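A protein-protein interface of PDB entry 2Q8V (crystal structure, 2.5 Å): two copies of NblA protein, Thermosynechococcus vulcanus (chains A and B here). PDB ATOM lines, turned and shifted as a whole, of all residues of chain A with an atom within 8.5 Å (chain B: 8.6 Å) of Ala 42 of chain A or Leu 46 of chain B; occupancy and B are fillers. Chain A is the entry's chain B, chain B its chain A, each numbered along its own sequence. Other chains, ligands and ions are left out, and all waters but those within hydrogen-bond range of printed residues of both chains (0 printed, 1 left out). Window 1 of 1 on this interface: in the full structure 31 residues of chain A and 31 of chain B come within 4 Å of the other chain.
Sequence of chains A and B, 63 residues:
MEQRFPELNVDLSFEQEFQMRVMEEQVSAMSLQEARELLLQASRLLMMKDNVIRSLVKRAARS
Printed residues of chain A that touch a printed residue of chain B: Met 20, Met 23, Ala 35, Leu 38, Leu 39, Leu 40, Ala 42, Ser 43, Arg 44, Leu 45, Leu 46, Met 47, Lys 49 and Asp 50. Hydrophobic or aromatic side chains of chain A that line the printed part of chain B: Met 20, Met 23, Leu 38, Leu 39, Leu 40, Ala 42, Leu 45, Leu 46 and Met 47. Hydrophobic or aromatic side chains of chain B within 4 Å of the printed part of chain A: Met 20, Met 23, Leu 39, Leu 40, Ala 42, Leu 46 and Met 47. Among the printed residues, 24 pairs touch across the chains. Among the printed residues, Asp or Glu carboxylates within 4 Å of a Lys or Arg side-chain nitrogen of the other chain: Lys 49 of chain A with Asp 50 of chain B (3.2 Å) and Asp 50 of chain A with Lys 49 of chain B (3.3 Å).
Ala 42 of chain A touches just these residues of chain B: Ala 42 and Leu 46. Leu 46 of chain B touches just these residues of chain A: Ala 42 (3.8 Å), Leu 45 (3.7 Å), Leu 46 (3.5 Å) and Lys 49 (3.4 Å). Printed residues of chain B within 4 Å of Leu 46 of chain A: Leu 46 and Lys 49. Of the printed residues of chain A, Leu 40 of chain B touches Met 20 (3.9 Å) and Met 23 (3.9 Å). The nearest residue of chain A that does not touch Leu 46 of chain B is Ser 43 of chain A (5.9 Å).
SD of Met 20 of chain A touches CE of Met 47 of chain B, at 3.9 Å. Met 47 of chain B touches Met 23 of chain A. CB of Leu 38 of chain A touches CD1 of Leu 39 of chain B, at 3.8 Å. CD2 of Leu 39 of chain A touches CE of Met 23 of chain B, at 3.8 Å. Leu 39 of chain B touches Leu 39 of chain A (CG to N, 3.8 Å). Met 23 of chain B touches Leu 40 of chain A. CB of Ala 42 of chain A touches CD1 of Leu 46 of chain B, 3.8 Å away. CD2 of Leu 46 of chain A touches CD2 of Leu 46 of chain B, at 3.5 Å. Lys 49 of chain A touches Leu 46 of chain B. CD of Lys 49 of chain A touches CB of Lys 49 of chain B, at 3.6 Å.
Met 23 of chain A touches Ser 43 of chain B, and with the chains exchanged Ser 43 of chain A touches Met 23 of chain B. Leu 38 of chain A touches Leu 39 of chain B, but with the chains exchanged Leu 39 of chain A does not touch Leu 38 of chain B (4.1 Å). Ala 42 of chain A touches its own counterpart, Ala 42 of chain B. Lys 49 of chain B touches its own counterpart, Lys 49 of chain A. 15 positions are printed for both chains.
The backbone NH of Arg 44 of chain B is in hydrogen-bond range of the side-chain sulfur of Met 20 of chain A (3.7 Å). NZ of Lys 49 of chain B lies within salt-bridge range of OD1 of Asp 50 of chain A (3.3 Å). OD1 of Asp 50 of chain B is in salt-bridge range of NZ of Lys 49 of chain A, at 3.2 Å.
O of Leu 39 of chain B is in hydrogen-bond range of OG of Ser 43 of chain B (2.8 Å). O of Leu 39 of chain A lies within hydrogen-bond range of OG of Ser 43 of chain A.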
ATOM      1  N   SER A  13      17.339  38.008  10.346  1.00  0.00           N
ATOM      2  CA  SER A  13      17.155  36.913   9.416  1.00  0.00           C
ATOM      3  C   SER A  13      15.963  37.104   8.457  1.00  0.00           C
ATOM      4  O   SER A  13      14.954  37.626   8.850  1.00  0.00           O
ATOM      5  CB  SER A  13      17.092  35.586  10.167  1.00  0.00           C
ATOM      6  OG  SER A  13      18.349  35.200  10.703  1.00  0.00           O
ATOM      7  N   MET A  20      15.337  28.299  10.607  1.00  0.00           N
ATOM      8  CA  MET A  20      15.596  28.178  12.042  1.00  0.00           C
ATOM      9  C   MET A  20      14.593  27.285  12.769  1.00  0.00           C
ATOM     10  O   MET A  20      14.987  26.552  13.681  1.00  0.00           O
ATOM     11  CB  MET A  20      15.638  29.543  12.728  1.00  0.00           C
ATOM     12  CG  MET A  20      17.005  30.231  12.718  1.00  0.00           C
ATOM     13  SD  MET A  20      18.431  29.250  13.267  1.00  0.00           S
ATOM     14  CE  MET A  20      17.905  28.614  14.860  1.00  0.00           C
ATOM     15  N   MET A  23      15.497  23.758  11.813  1.00  0.00           N
ATOM     16  CA  MET A  23      16.710  23.461  12.561  1.00  0.00           C
ATOM     17  C   MET A  23      16.394  23.157  14.026  1.00  0.00           C
ATOM     18  O   MET A  23      16.940  22.217  14.590  1.00  0.00           O
ATOM     19  CB  MET A  23      17.692  24.638  12.455  1.00  0.00           C
ATOM     20  CG  MET A  23      19.129  24.274  12.019  1.00  0.00           C
ATOM     21  SD  MET A  23      19.804  25.383  10.708  1.00  0.00           S
ATOM     22  CE  MET A  23      19.057  24.684   9.211  1.00  0.00           C
ATOM     23  N   ALA A  35      25.082  16.431  18.076  1.00  0.00           N
ATOM     24  CA  ALA A  35      25.030  17.817  18.494  1.00  0.00           C
ATOM     25  C   ALA A  35      26.449  18.346  18.621  1.00  0.00           C
ATOM     26  O   ALA A  35      26.734  19.452  18.167  1.00  0.00           O
ATOM     27  CB  ALA A  35      24.272  17.957  19.801  1.00  0.00           C
ATOM     28  N   ARG A  36      27.334  17.536  19.202  1.00  0.00           N
ATOM     29  CA  ARG A  36      28.757  17.869  19.339  1.00  0.00           C
ATOM     30  C   ARG A  36      29.499  18.001  18.005  1.00  0.00           C
ATOM     31  O   ARG A  36      30.271  18.956  17.808  1.00  0.00           O
ATOM     32  CB  ARG A  36      29.479  16.832  20.209  1.00  0.00           C
ATOM     33  CG  ARG A  36      29.206  16.949  21.693  1.00  0.00           C
ATOM     34  CD  ARG A  36      30.003  15.943  22.491  1.00  0.00           C
ATOM     35  NE  ARG A  36      29.687  16.061  23.915  1.00  0.00           N
ATOM     36  CZ  ARG A  36      30.088  15.215  24.860  1.00  0.00           C
ATOM     37  NH1 ARG A  36      30.834  14.171  24.546  1.00  0.00           N
ATOM     38  NH2 ARG A  36      29.730  15.409  26.123  1.00  0.00           N
ATOM     39  N   GLU A  37      29.285  17.037  17.107  1.00  0.00           N
ATOM     40  CA  GLU A  37      29.936  17.040  15.795  1.00  0.00           C
ATOM     41  C   GLU A  37      29.516  18.266  15.007  1.00  0.00           C
ATOM     42  O   GLU A  37      30.370  19.015  14.517  1.00  0.00           O
ATOM     43  CB  GLU A  37      29.618  15.774  15.005  1.00  0.00           C
ATOM     44  CG  GLU A  37      30.592  14.629  15.238  1.00  0.00           C
ATOM     45  CD  GLU A  37      30.130  13.307  14.596  1.00  0.00           C
ATOM     46  OE1 GLU A  37      29.005  13.250  14.036  1.00  0.00           O
ATOM     47  OE2 GLU A  37      30.889  12.306  14.672  1.00  0.00           O
ATOM     48  N   LEU A  38      28.202  18.479  14.928  1.00  0.00           N
ATOM     49  CA  LEU A  38      27.620  19.585  14.169  1.00  0.00           C
ATOM     50  C   LEU A  38      28.024  20.960  14.719  1.00  0.00           C
ATOM     51  O   LEU A  38      28.365  21.885  13.958  1.00  0.00           O
ATOM     52  CB  LEU A  38      26.096  19.421  14.096  1.00  0.00           C
ATOM     53  CG  LEU A  38      25.514  18.734  12.834  1.00  0.00           C
ATOM     54  CD1 LEU A  38      26.497  17.854  12.052  1.00  0.00           C
ATOM     55  CD2 LEU A  38      24.228  17.958  13.145  1.00  0.00           C
ATOM     56  N   LEU A  39      28.009  21.072  16.046  1.00  0.00           N
ATOM     57  CA  LEU A  39      28.436  22.273  16.727  1.00  0.00           C
ATOM     58  C   LEU A  39      29.855  22.582  16.321  1.00  0.00           C
ATOM     59  O   LEU A  39      30.200  23.748  16.050  1.00  0.00           O
ATOM     60  CB  LEU A  39      28.418  22.057  18.233  1.00  0.00           C
ATOM     61  CG  LEU A  39      28.267  23.226  19.219  1.00  0.00           C
ATOM     62  CD1 LEU A  39      29.039  22.915  20.479  1.00  0.00           C
ATOM     63  CD2 LEU A  39      28.657  24.601  18.684  1.00  0.00           C
ATOM     64  N   LEU A  40      30.690  21.549  16.296  1.00  0.00           N
ATOM     65  CA  LEU A  40      32.078  21.758  15.955  1.00  0.00           C
ATOM     66  C   LEU A  40      32.191  22.217  14.505  1.00  0.00           C
ATOM     67  O   LEU A  40      32.961  23.136  14.190  1.00  0.00           O
ATOM     68  CB  LEU A  40      32.900  20.498  16.231  1.00  0.00           C
ATOM     69  CG  LEU A  40      33.351  20.409  17.693  1.00  0.00           C
ATOM     70  CD1 LEU A  40      33.820  18.984  18.053  1.00  0.00           C
ATOM     71  CD2 LEU A  40      34.439  21.460  17.958  1.00  0.00           C
ATOM     72  N   GLN A  41      31.397  21.607  13.634  1.00  0.00           N
ATOM     73  CA  GLN A  41      31.399  21.994  12.245  1.00  0.00           C
ATOM     74  C   GLN A  41      30.980  23.444  12.087  1.00  0.00           C
ATOM     75  O   GLN A  41      31.653  24.203  11.373  1.00  0.00           O
ATOM     76  CB  GLN A  41      30.490  21.092  11.414  1.00  0.00           C
ATOM     77  CG  GLN A  41      31.192  19.884  10.841  1.00  0.00           C
ATOM     78  CD  GLN A  41      30.371  19.215   9.746  1.00  0.00           C
ATOM     79  OE1 GLN A  41      29.952  19.859   8.764  1.00  0.00           O
ATOM     80  NE2 GLN A  41      30.132  17.909   9.911  1.00  0.00           N
ATOM     81  N   ALA A  42      29.884  23.817  12.752  1.00  0.00           N
ATOM     82  CA  ALA A  42      29.373  25.185  12.713  1.00  0.00           C
ATOM     83  C   ALA A  42      30.456  26.178  13.139  1.00  0.00           C
ATOM     84  O   ALA A  42      30.678  27.201  12.470  1.00  0.00           O
ATOM     85  CB  ALA A  42      28.115  25.330  13.585  1.00  0.00           C
ATOM     86  N   SER A  43      31.149  25.856  14.233  1.00  0.00           N
ATOM     87  CA  SER A  43      32.225  26.714  14.742  1.00  0.00           C
ATOM     88  C   SER A  43      33.352  26.879  13.725  1.00  0.00           C
ATOM     89  O   SER A  43      33.955  27.952  13.632  1.00  0.00           O
ATOM     90  CB  SER A  43      32.775  26.159  16.055  1.00  0.00           C
ATOM     91  OG  SER A  43      31.746  26.058  17.030  1.00  0.00           O
ATOM     92  N   ARG A  44      33.630  25.811  12.974  1.00  0.00           N
ATOM     93  CA  ARG A  44      34.581  25.862  11.860  1.00  0.00           C
ATOM     94  C   ARG A  44      34.087  26.772  10.733  1.00  0.00           C
ATOM     95  O   ARG A  44      34.846  27.592  10.216  1.00  0.00           O
ATOM     96  CB  ARG A  44      34.850  24.457  11.334  1.00  0.00           C
ATOM     97  CG  ARG A  44      35.678  24.400  10.069  1.00  0.00           C
ATOM     98  CD  ARG A  44      36.112  22.961   9.786  1.00  0.00           C
ATOM     99  NE  ARG A  44      37.194  22.540  10.680  1.00  0.00           N
ATOM    100  CZ  ARG A  44      38.487  22.760  10.449  1.00  0.00           C
ATOM    101  NH1 ARG A  44      38.869  23.394   9.355  1.00  0.00           N
ATOM    102  NH2 ARG A  44      39.402  22.355  11.321  1.00  0.00           N
ATOM    103  N   LEU A  45      32.814  26.634  10.367  1.00  0.00           N
ATOM    104  CA  LEU A  45      32.205  27.505   9.361  1.00  0.00           C
ATOM    105  C   LEU A  45      32.155  28.980   9.775  1.00  0.00           C
ATOM    106  O   LEU A  45      32.364  29.866   8.938  1.00  0.00           O
ATOM    107  CB  LEU A  45      30.808  27.007   8.986  1.00  0.00           C
ATOM    108  CG  LEU A  45      30.731  25.708   8.192  1.00  0.00           C
ATOM    109  CD1 LEU A  45      29.300  25.311   8.051  1.00  0.00           C
ATOM    110  CD2 LEU A  45      31.300  25.919   6.809  1.00  0.00           C
ATOM    111  N   LEU A  46      31.883  29.239  11.050  1.00  0.00           N
ATOM    112  CA  LEU A  46      31.869  30.607  11.563  1.00  0.00           C
ATOM    113  C   LEU A  46      33.188  31.325  11.329  1.00  0.00           C
ATOM    114  O   LEU A  46      33.204  32.482  10.915  1.00  0.00           O
ATOM    115  CB  LEU A  46      31.524  30.642  13.056  1.00  0.00           C
ATOM    116  CG  LEU A  46      30.052  30.338  13.362  1.00  0.00           C
ATOM    117  CD1 LEU A  46      29.800  30.257  14.859  1.00  0.00           C
ATOM    118  CD2 LEU A  46      29.183  31.403  12.706  1.00  0.00           C
ATOM    119  N   MET A  47      34.293  30.630  11.607  1.00  0.00           N
ATOM    120  CA  MET A  47      35.639  31.161  11.398  1.00  0.00           C
ATOM    121  C   MET A  47      35.943  31.374   9.908  1.00  0.00           C
ATOM    122  O   MET A  47      36.479  32.419   9.519  1.00  0.00           O
ATOM    123  CB  MET A  47      36.666  30.236  12.052  1.00  0.00           C
ATOM    124  CG  MET A  47      36.793  30.398  13.585  1.00  0.00           C
ATOM    125  SD  MET A  47      38.029  29.297  14.348  1.00  0.00           S
ATOM    126  CE  MET A  47      36.959  28.195  15.275  1.00  0.00           C
ATOM    127  N   MET A  48      35.582  30.388   9.084  1.00  0.00           N
ATOM    128  CA  MET A  48      35.649  30.518   7.617  1.00  0.00           C
ATOM    129  C   MET A  48      34.890  31.747   7.097  1.00  0.00           C
ATOM    130  O   MET A  48      35.462  32.575   6.385  1.00  0.00           O
ATOM    131  CB  MET A  48      35.154  29.243   6.935  1.00  0.00           C
ATOM    132  CG  MET A  48      36.118  28.045   7.079  1.00  0.00           C
ATOM    133  SD  MET A  48      35.318  26.446   6.836  1.00  0.00           S
ATOM    134  CE  MET A  48      34.972  26.465   5.073  1.00  0.00           C
ATOM    135  N   LYS A  49      33.623  31.887   7.485  1.00  0.00           N
ATOM    136  CA  LYS A  49      32.848  33.107   7.186  1.00  0.00           C
ATOM    137  C   LYS A  49      33.469  34.385   7.746  1.00  0.00           C
ATOM    138  O   LYS A  49      33.411  35.431   7.098  1.00  0.00           O
ATOM    139  CB  LYS A  49      31.403  32.990   7.671  1.00  0.00           C
ATOM    140  CG  LYS A  49      30.572  31.954   6.942  1.00  0.00           C
ATOM    141  CD  LYS A  49      29.115  32.204   7.248  1.00  0.00           C
ATOM    142  CE  LYS A  49      28.242  30.965   7.092  1.00  0.00           C
ATOM    143  NZ  LYS A  49      28.428  30.327   5.795  1.00  0.00           N
ATOM    144  N   ASP A  50      34.058  34.313   8.936  1.00  0.00           N
ATOM    145  CA  ASP A  50      34.811  35.445   9.470  1.00  0.00           C
ATOM    146  C   ASP A  50      35.943  35.822   8.526  1.00  0.00           C
ATOM    147  O   ASP A  50      36.154  37.002   8.240  1.00  0.00           O
ATOM    148  CB  ASP A  50      35.372  35.145  10.860  1.00  0.00           C
ATOM    149  CG  ASP A  50      34.428  35.572  11.987  1.00  0.00           C
ATOM    150  OD1 ASP A  50      33.637  36.531  11.793  1.00  0.00           O
ATOM    151  OD2 ASP A  50      34.495  34.943  13.077  1.00  0.00           O
ATOM    152  N   MET B  20      40.157  25.839  17.190  1.00  0.00           N
ATOM    153  CA  MET B  20      39.360  24.642  16.970  1.00  0.00           C
ATOM    154  C   MET B  20      39.703  23.525  17.949  1.00  0.00           C
ATOM    155  O   MET B  20      38.810  22.767  18.336  1.00  0.00           O
ATOM    156  CB  MET B  20      39.481  24.142  15.537  1.00  0.00           C
ATOM    157  CG  MET B  20      38.578  24.859  14.539  1.00  0.00           C
ATOM    158  SD  MET B  20      36.806  24.838  14.937  1.00  0.00           S
ATOM    159  CE  MET B  20      36.384  23.100  14.734  1.00  0.00           C
ATOM    160  N   MET B  23      37.910  24.568  21.122  1.00  0.00           N
ATOM    161  CA  MET B  23      36.491  24.243  20.940  1.00  0.00           C
ATOM    162  C   MET B  23      36.183  22.741  21.065  1.00  0.00           C
ATOM    163  O   MET B  23      35.185  22.369  21.665  1.00  0.00           O
ATOM    164  CB  MET B  23      35.929  24.818  19.627  1.00  0.00           C
ATOM    165  CG  MET B  23      34.963  26.009  19.815  1.00  0.00           C
ATOM    166  SD  MET B  23      33.579  25.774  21.011  1.00  0.00           S
ATOM    167  CE  MET B  23      32.212  25.339  19.955  1.00  0.00           C
ATOM    168  N   LEU B  38      23.813  25.512  21.820  1.00  0.00           N
ATOM    169  CA  LEU B  38      24.950  26.192  21.215  1.00  0.00           C
ATOM    170  C   LEU B  38      24.964  25.970  19.710  1.00  0.00           C
ATOM    171  O   LEU B  38      25.303  26.883  18.942  1.00  0.00           O
ATOM    172  CB  LEU B  38      26.263  25.763  21.873  1.00  0.00           C
ATOM    173  CG  LEU B  38      26.984  26.728  22.852  1.00  0.00           C
ATOM    174  CD1 LEU B  38      26.084  27.620  23.705  1.00  0.00           C
ATOM    175  CD2 LEU B  38      27.899  25.956  23.771  1.00  0.00           C
ATOM    176  N   LEU B  39      24.553  24.777  19.295  1.00  0.00           N
ATOM    177  CA  LEU B  39      24.374  24.459  17.880  1.00  0.00           C
ATOM    178  C   LEU B  39      23.357  25.376  17.226  1.00  0.00           C
ATOM    179  O   LEU B  39      23.549  25.810  16.084  1.00  0.00           O
ATOM    180  CB  LEU B  39      23.907  23.020  17.692  1.00  0.00           C
ATOM    181  CG  LEU B  39      24.431  22.205  16.502  1.00  0.00           C
ATOM    182  CD1 LEU B  39      23.465  21.092  16.231  1.00  0.00           C
ATOM    183  CD2 LEU B  39      24.632  22.989  15.234  1.00  0.00           C
ATOM    184  N   LEU B  40      22.271  25.660  17.943  1.00  0.00           N
ATOM    185  CA  LEU B  40      21.228  26.541  17.440  1.00  0.00           C
ATOM    186  C   LEU B  40      21.687  27.975  17.417  1.00  0.00           C
ATOM    187  O   LEU B  40      21.406  28.705  16.471  1.00  0.00           O
ATOM    188  CB  LEU B  40      19.979  26.424  18.290  1.00  0.00           C
ATOM    189  CG  LEU B  40      19.201  25.144  18.038  1.00  0.00           C
ATOM    190  CD1 LEU B  40      17.982  25.128  18.953  1.00  0.00           C
ATOM    191  CD2 LEU B  40      18.793  25.055  16.564  1.00  0.00           C
ATOM    192  N   GLN B  41      22.381  28.388  18.469  1.00  0.00           N
ATOM    193  CA  GLN B  41      22.961  29.724  18.492  1.00  0.00           C
ATOM    194  C   GLN B  41      23.890  29.898  17.299  1.00  0.00           C
ATOM    195  O   GLN B  41      23.798  30.900  16.594  1.00  0.00           O
ATOM    196  CB  GLN B  41      23.709  29.992  19.802  1.00  0.00           C
ATOM    197  CG  GLN B  41      22.808  30.440  20.921  1.00  0.00           C
ATOM    198  CD  GLN B  41      23.538  30.568  22.241  1.00  0.00           C
ATOM    199  OE1 GLN B  41      24.696  30.987  22.279  1.00  0.00           O
ATOM    200  NE2 GLN B  41      22.857  30.213  23.339  1.00  0.00           N
ATOM    201  N   ALA B  42      24.756  28.910  17.075  1.00  0.00           N
ATOM    202  CA  ALA B  42      25.722  28.942  15.960  1.00  0.00           C
ATOM    203  C   ALA B  42      25.012  28.973  14.619  1.00  0.00           C
ATOM    204  O   ALA B  42      25.441  29.685  13.708  1.00  0.00           O
ATOM    205  CB  ALA B  42      26.687  27.756  16.029  1.00  0.00           C
ATOM    206  N   SER B  43      23.914  28.213  14.525  1.00  0.00           N
ATOM    207  CA  SER B  43      23.122  28.097  13.306  1.00  0.00           C
ATOM    208  C   SER B  43      22.519  29.427  12.938  1.00  0.00           C
ATOM    209  O   SER B  43      22.505  29.795  11.762  1.00  0.00           O
ATOM    210  CB  SER B  43      22.006  27.082  13.477  1.00  0.00           C
ATOM    211  OG  SER B  43      22.509  25.764  13.459  1.00  0.00           O
ATOM    212  N   ARG B  44      22.007  30.136  13.934  1.00  0.00           N
ATOM    213  CA  ARG B  44      21.489  31.477  13.723  1.00  0.00           C
ATOM    214  C   ARG B  44      22.611  32.441  13.328  1.00  0.00           C
ATOM    215  O   ARG B  44      22.459  33.250  12.413  1.00  0.00           O
ATOM    216  CB  ARG B  44      20.762  31.975  14.980  1.00  0.00           C
ATOM    217  CG  ARG B  44      20.388  33.458  14.944  1.00  0.00           C
ATOM    218  CD  ARG B  44      19.614  33.905  16.197  1.00  0.00           C
ATOM    219  NE  ARG B  44      18.435  33.068  16.437  1.00  0.00           N
ATOM    220  CZ  ARG B  44      17.233  33.279  15.900  1.00  0.00           C
ATOM    221  NH1 ARG B  44      17.025  34.314  15.079  1.00  0.00           N
ATOM    222  NH2 ARG B  44      16.231  32.447  16.192  1.00  0.00           N
ATOM    223  N   LEU B  45      23.738  32.348  14.012  1.00  0.00           N
ATOM    224  CA  LEU B  45      24.872  33.209  13.702  1.00  0.00           C
ATOM    225  C   LEU B  45      25.429  32.939  12.297  1.00  0.00           C
ATOM    226  O   LEU B  45      25.920  33.855  11.644  1.00  0.00           O
ATOM    227  CB  LEU B  45      25.972  33.044  14.749  1.00  0.00           C
ATOM    228  CG  LEU B  45      26.470  34.278  15.511  1.00  0.00           C
ATOM    229  CD1 LEU B  45      27.767  33.928  16.261  1.00  0.00           C
ATOM    230  CD2 LEU B  45      26.692  35.471  14.581  1.00  0.00           C
ATOM    231  N   LEU B  46      25.350  31.689  11.841  1.00  0.00           N
ATOM    232  CA  LEU B  46      25.782  31.337  10.488  1.00  0.00           C
ATOM    233  C   LEU B  46      24.970  32.091   9.437  1.00  0.00           C
ATOM    234  O   LEU B  46      25.532  32.675   8.506  1.00  0.00           O
ATOM    235  CB  LEU B  46      25.688  29.828  10.254  1.00  0.00           C
ATOM    236  CG  LEU B  46      26.844  29.039  10.858  1.00  0.00           C
ATOM    237  CD1 LEU B  46      26.531  27.560  10.892  1.00  0.00           C
ATOM    238  CD2 LEU B  46      28.102  29.288  10.087  1.00  0.00           C
ATOM    239  N   MET B  47      23.652  32.107   9.616  1.00  0.00           N
ATOM    240  CA  MET B  47      22.777  32.852   8.731  1.00  0.00           C
ATOM    241  C   MET B  47      23.023  34.341   8.793  1.00  0.00           C
ATOM    242  O   MET B  47      22.968  35.014   7.767  1.00  0.00           O
ATOM    243  CB  MET B  47      21.309  32.535   9.022  1.00  0.00           C
ATOM    244  CG  MET B  47      21.003  31.075   8.760  1.00  0.00           C
ATOM    245  SD  MET B  47      19.299  30.614   8.982  1.00  0.00           S
ATOM    246  CE  MET B  47      19.499  28.900   9.499  1.00  0.00           C
ATOM    247  N   MET B  48      23.286  34.864   9.988  1.00  0.00           N
ATOM    248  CA  MET B  48      23.561  36.292  10.144  1.00  0.00           C
ATOM    249  C   MET B  48      24.830  36.703   9.379  1.00  0.00           C
ATOM    250  O   MET B  48      24.883  37.771   8.770  1.00  0.00           O
ATOM    251  CB  MET B  48      23.659  36.667  11.624  1.00  0.00           C
ATOM    252  CG  MET B  48      22.314  36.708  12.357  1.00  0.00           C
ATOM    253  SD  MET B  48      22.453  37.104  14.136  1.00  0.00           S
ATOM    254  CE  MET B  48      23.094  38.787  14.128  1.00  0.00           C
ATOM    255  N   LYS B  49      25.839  35.845   9.389  1.00  0.00           N
ATOM    256  CA  LYS B  49      27.053  36.084   8.606  1.00  0.00           C
ATOM    257  C   LYS B  49      26.832  36.025   7.088  1.00  0.00           C
ATOM    258  O   LYS B  49      27.460  36.793   6.348  1.00  0.00           O
ATOM    259  CB  LYS B  49      28.184  35.145   9.058  1.00  0.00           C
ATOM    260  CG  LYS B  49      28.587  35.392  10.523  1.00  0.00           C
ATOM    261  CD  LYS B  49      29.915  34.787  10.881  1.00  0.00           C
ATOM    262  CE  LYS B  49      30.342  35.228  12.269  1.00  0.00           C
ATOM    263  NZ  LYS B  49      30.352  36.716  12.385  1.00  0.00           N
ATOM    264  N   ASP B  50      25.947  35.143   6.617  1.00  0.00           N
ATOM    265  CA  ASP B  50      25.589  35.138   5.188  1.00  0.00           C
ATOM    266  C   ASP B  50      25.027  36.484   4.759  1.00  0.00           C
ATOM    267  O   ASP B  50      25.344  36.972   3.667  1.00  0.00           O
ATOM    268  CB  ASP B  50      24.556  34.071   4.856  1.00  0.00           C
ATOM    269  CG  ASP B  50      25.119  32.677   4.939  1.00  0.00           C
ATOM    270  OD1 ASP B  50      26.319  32.490   4.601  1.00  0.00           O
ATOM    271  OD2 ASP B  50      24.356  31.763   5.339  1.00  0.00           O
ATOM    272  N   ASN B  51      24.184  37.064   5.623  1.00  0.00           N
ATOM    273  CA  ASN B  51      23.610  38.371   5.386  1.00  0.00           C
ATOM    274  C   ASN B  51      24.680  39.451   5.385  1.00  0.00           C
ATOM    275  O   ASN B  51      24.648  40.347   4.545  1.00  0.00           O
ATOM    276  CB  ASN B  51      22.507  38.669   6.403  1.00  0.00           C
ATOM    277  CG  ASN B  51      21.327  37.690   6.297  1.00  0.00           C
ATOM    278  OD1 ASN B  51      21.142  37.042   5.266  1.00  0.00           O
ATOM    279  ND2 ASN B  51      20.525  37.593   7.362  1.00  0.00           N
ATOM    280  N   VAL B  52      25.644  39.354   6.303  1.00  0.00           N
ATOM    281  CA  VAL B  52      26.777  40.302   6.327  1.00  0.00           C
ATOM    282  C   VAL B  52      27.584  40.212   5.035  1.00  0.00           C
ATOM    283  O   VAL B  52      27.946  41.235   4.464  1.00  0.00           O
ATOM    284  CB  VAL B  52      27.710  40.105   7.548  1.00  0.00           C
ATOM    285  CG1 VAL B  52      28.937  41.001   7.430  1.00  0.00           C
ATOM    286  CG2 VAL B  52      26.968  40.385   8.874  1.00  0.00           C
ATOM    287  N   ILE B  53      27.833  38.985   4.572  1.00  0.00           N
ATOM    288  CA  ILE B  53      28.552  38.729   3.326  1.00  0.00           C
ATOM    289  C   ILE B  53      27.771  39.262   2.132  1.00  0.00           C
ATOM    290  O   ILE B  53      28.345  39.846   1.214  1.00  0.00           O
ATOM    291  CB  ILE B  53      28.845  37.200   3.147  1.00  0.00           C
ATOM    292  CG1 ILE B  53      29.893  36.740   4.167  1.00  0.00           C
ATOM    293  CG2 ILE B  53      29.325  36.883   1.726  1.00  0.00           C
ATOM    294  CD1 ILE B  53      29.986  35.227   4.358  1.00  0.00           C
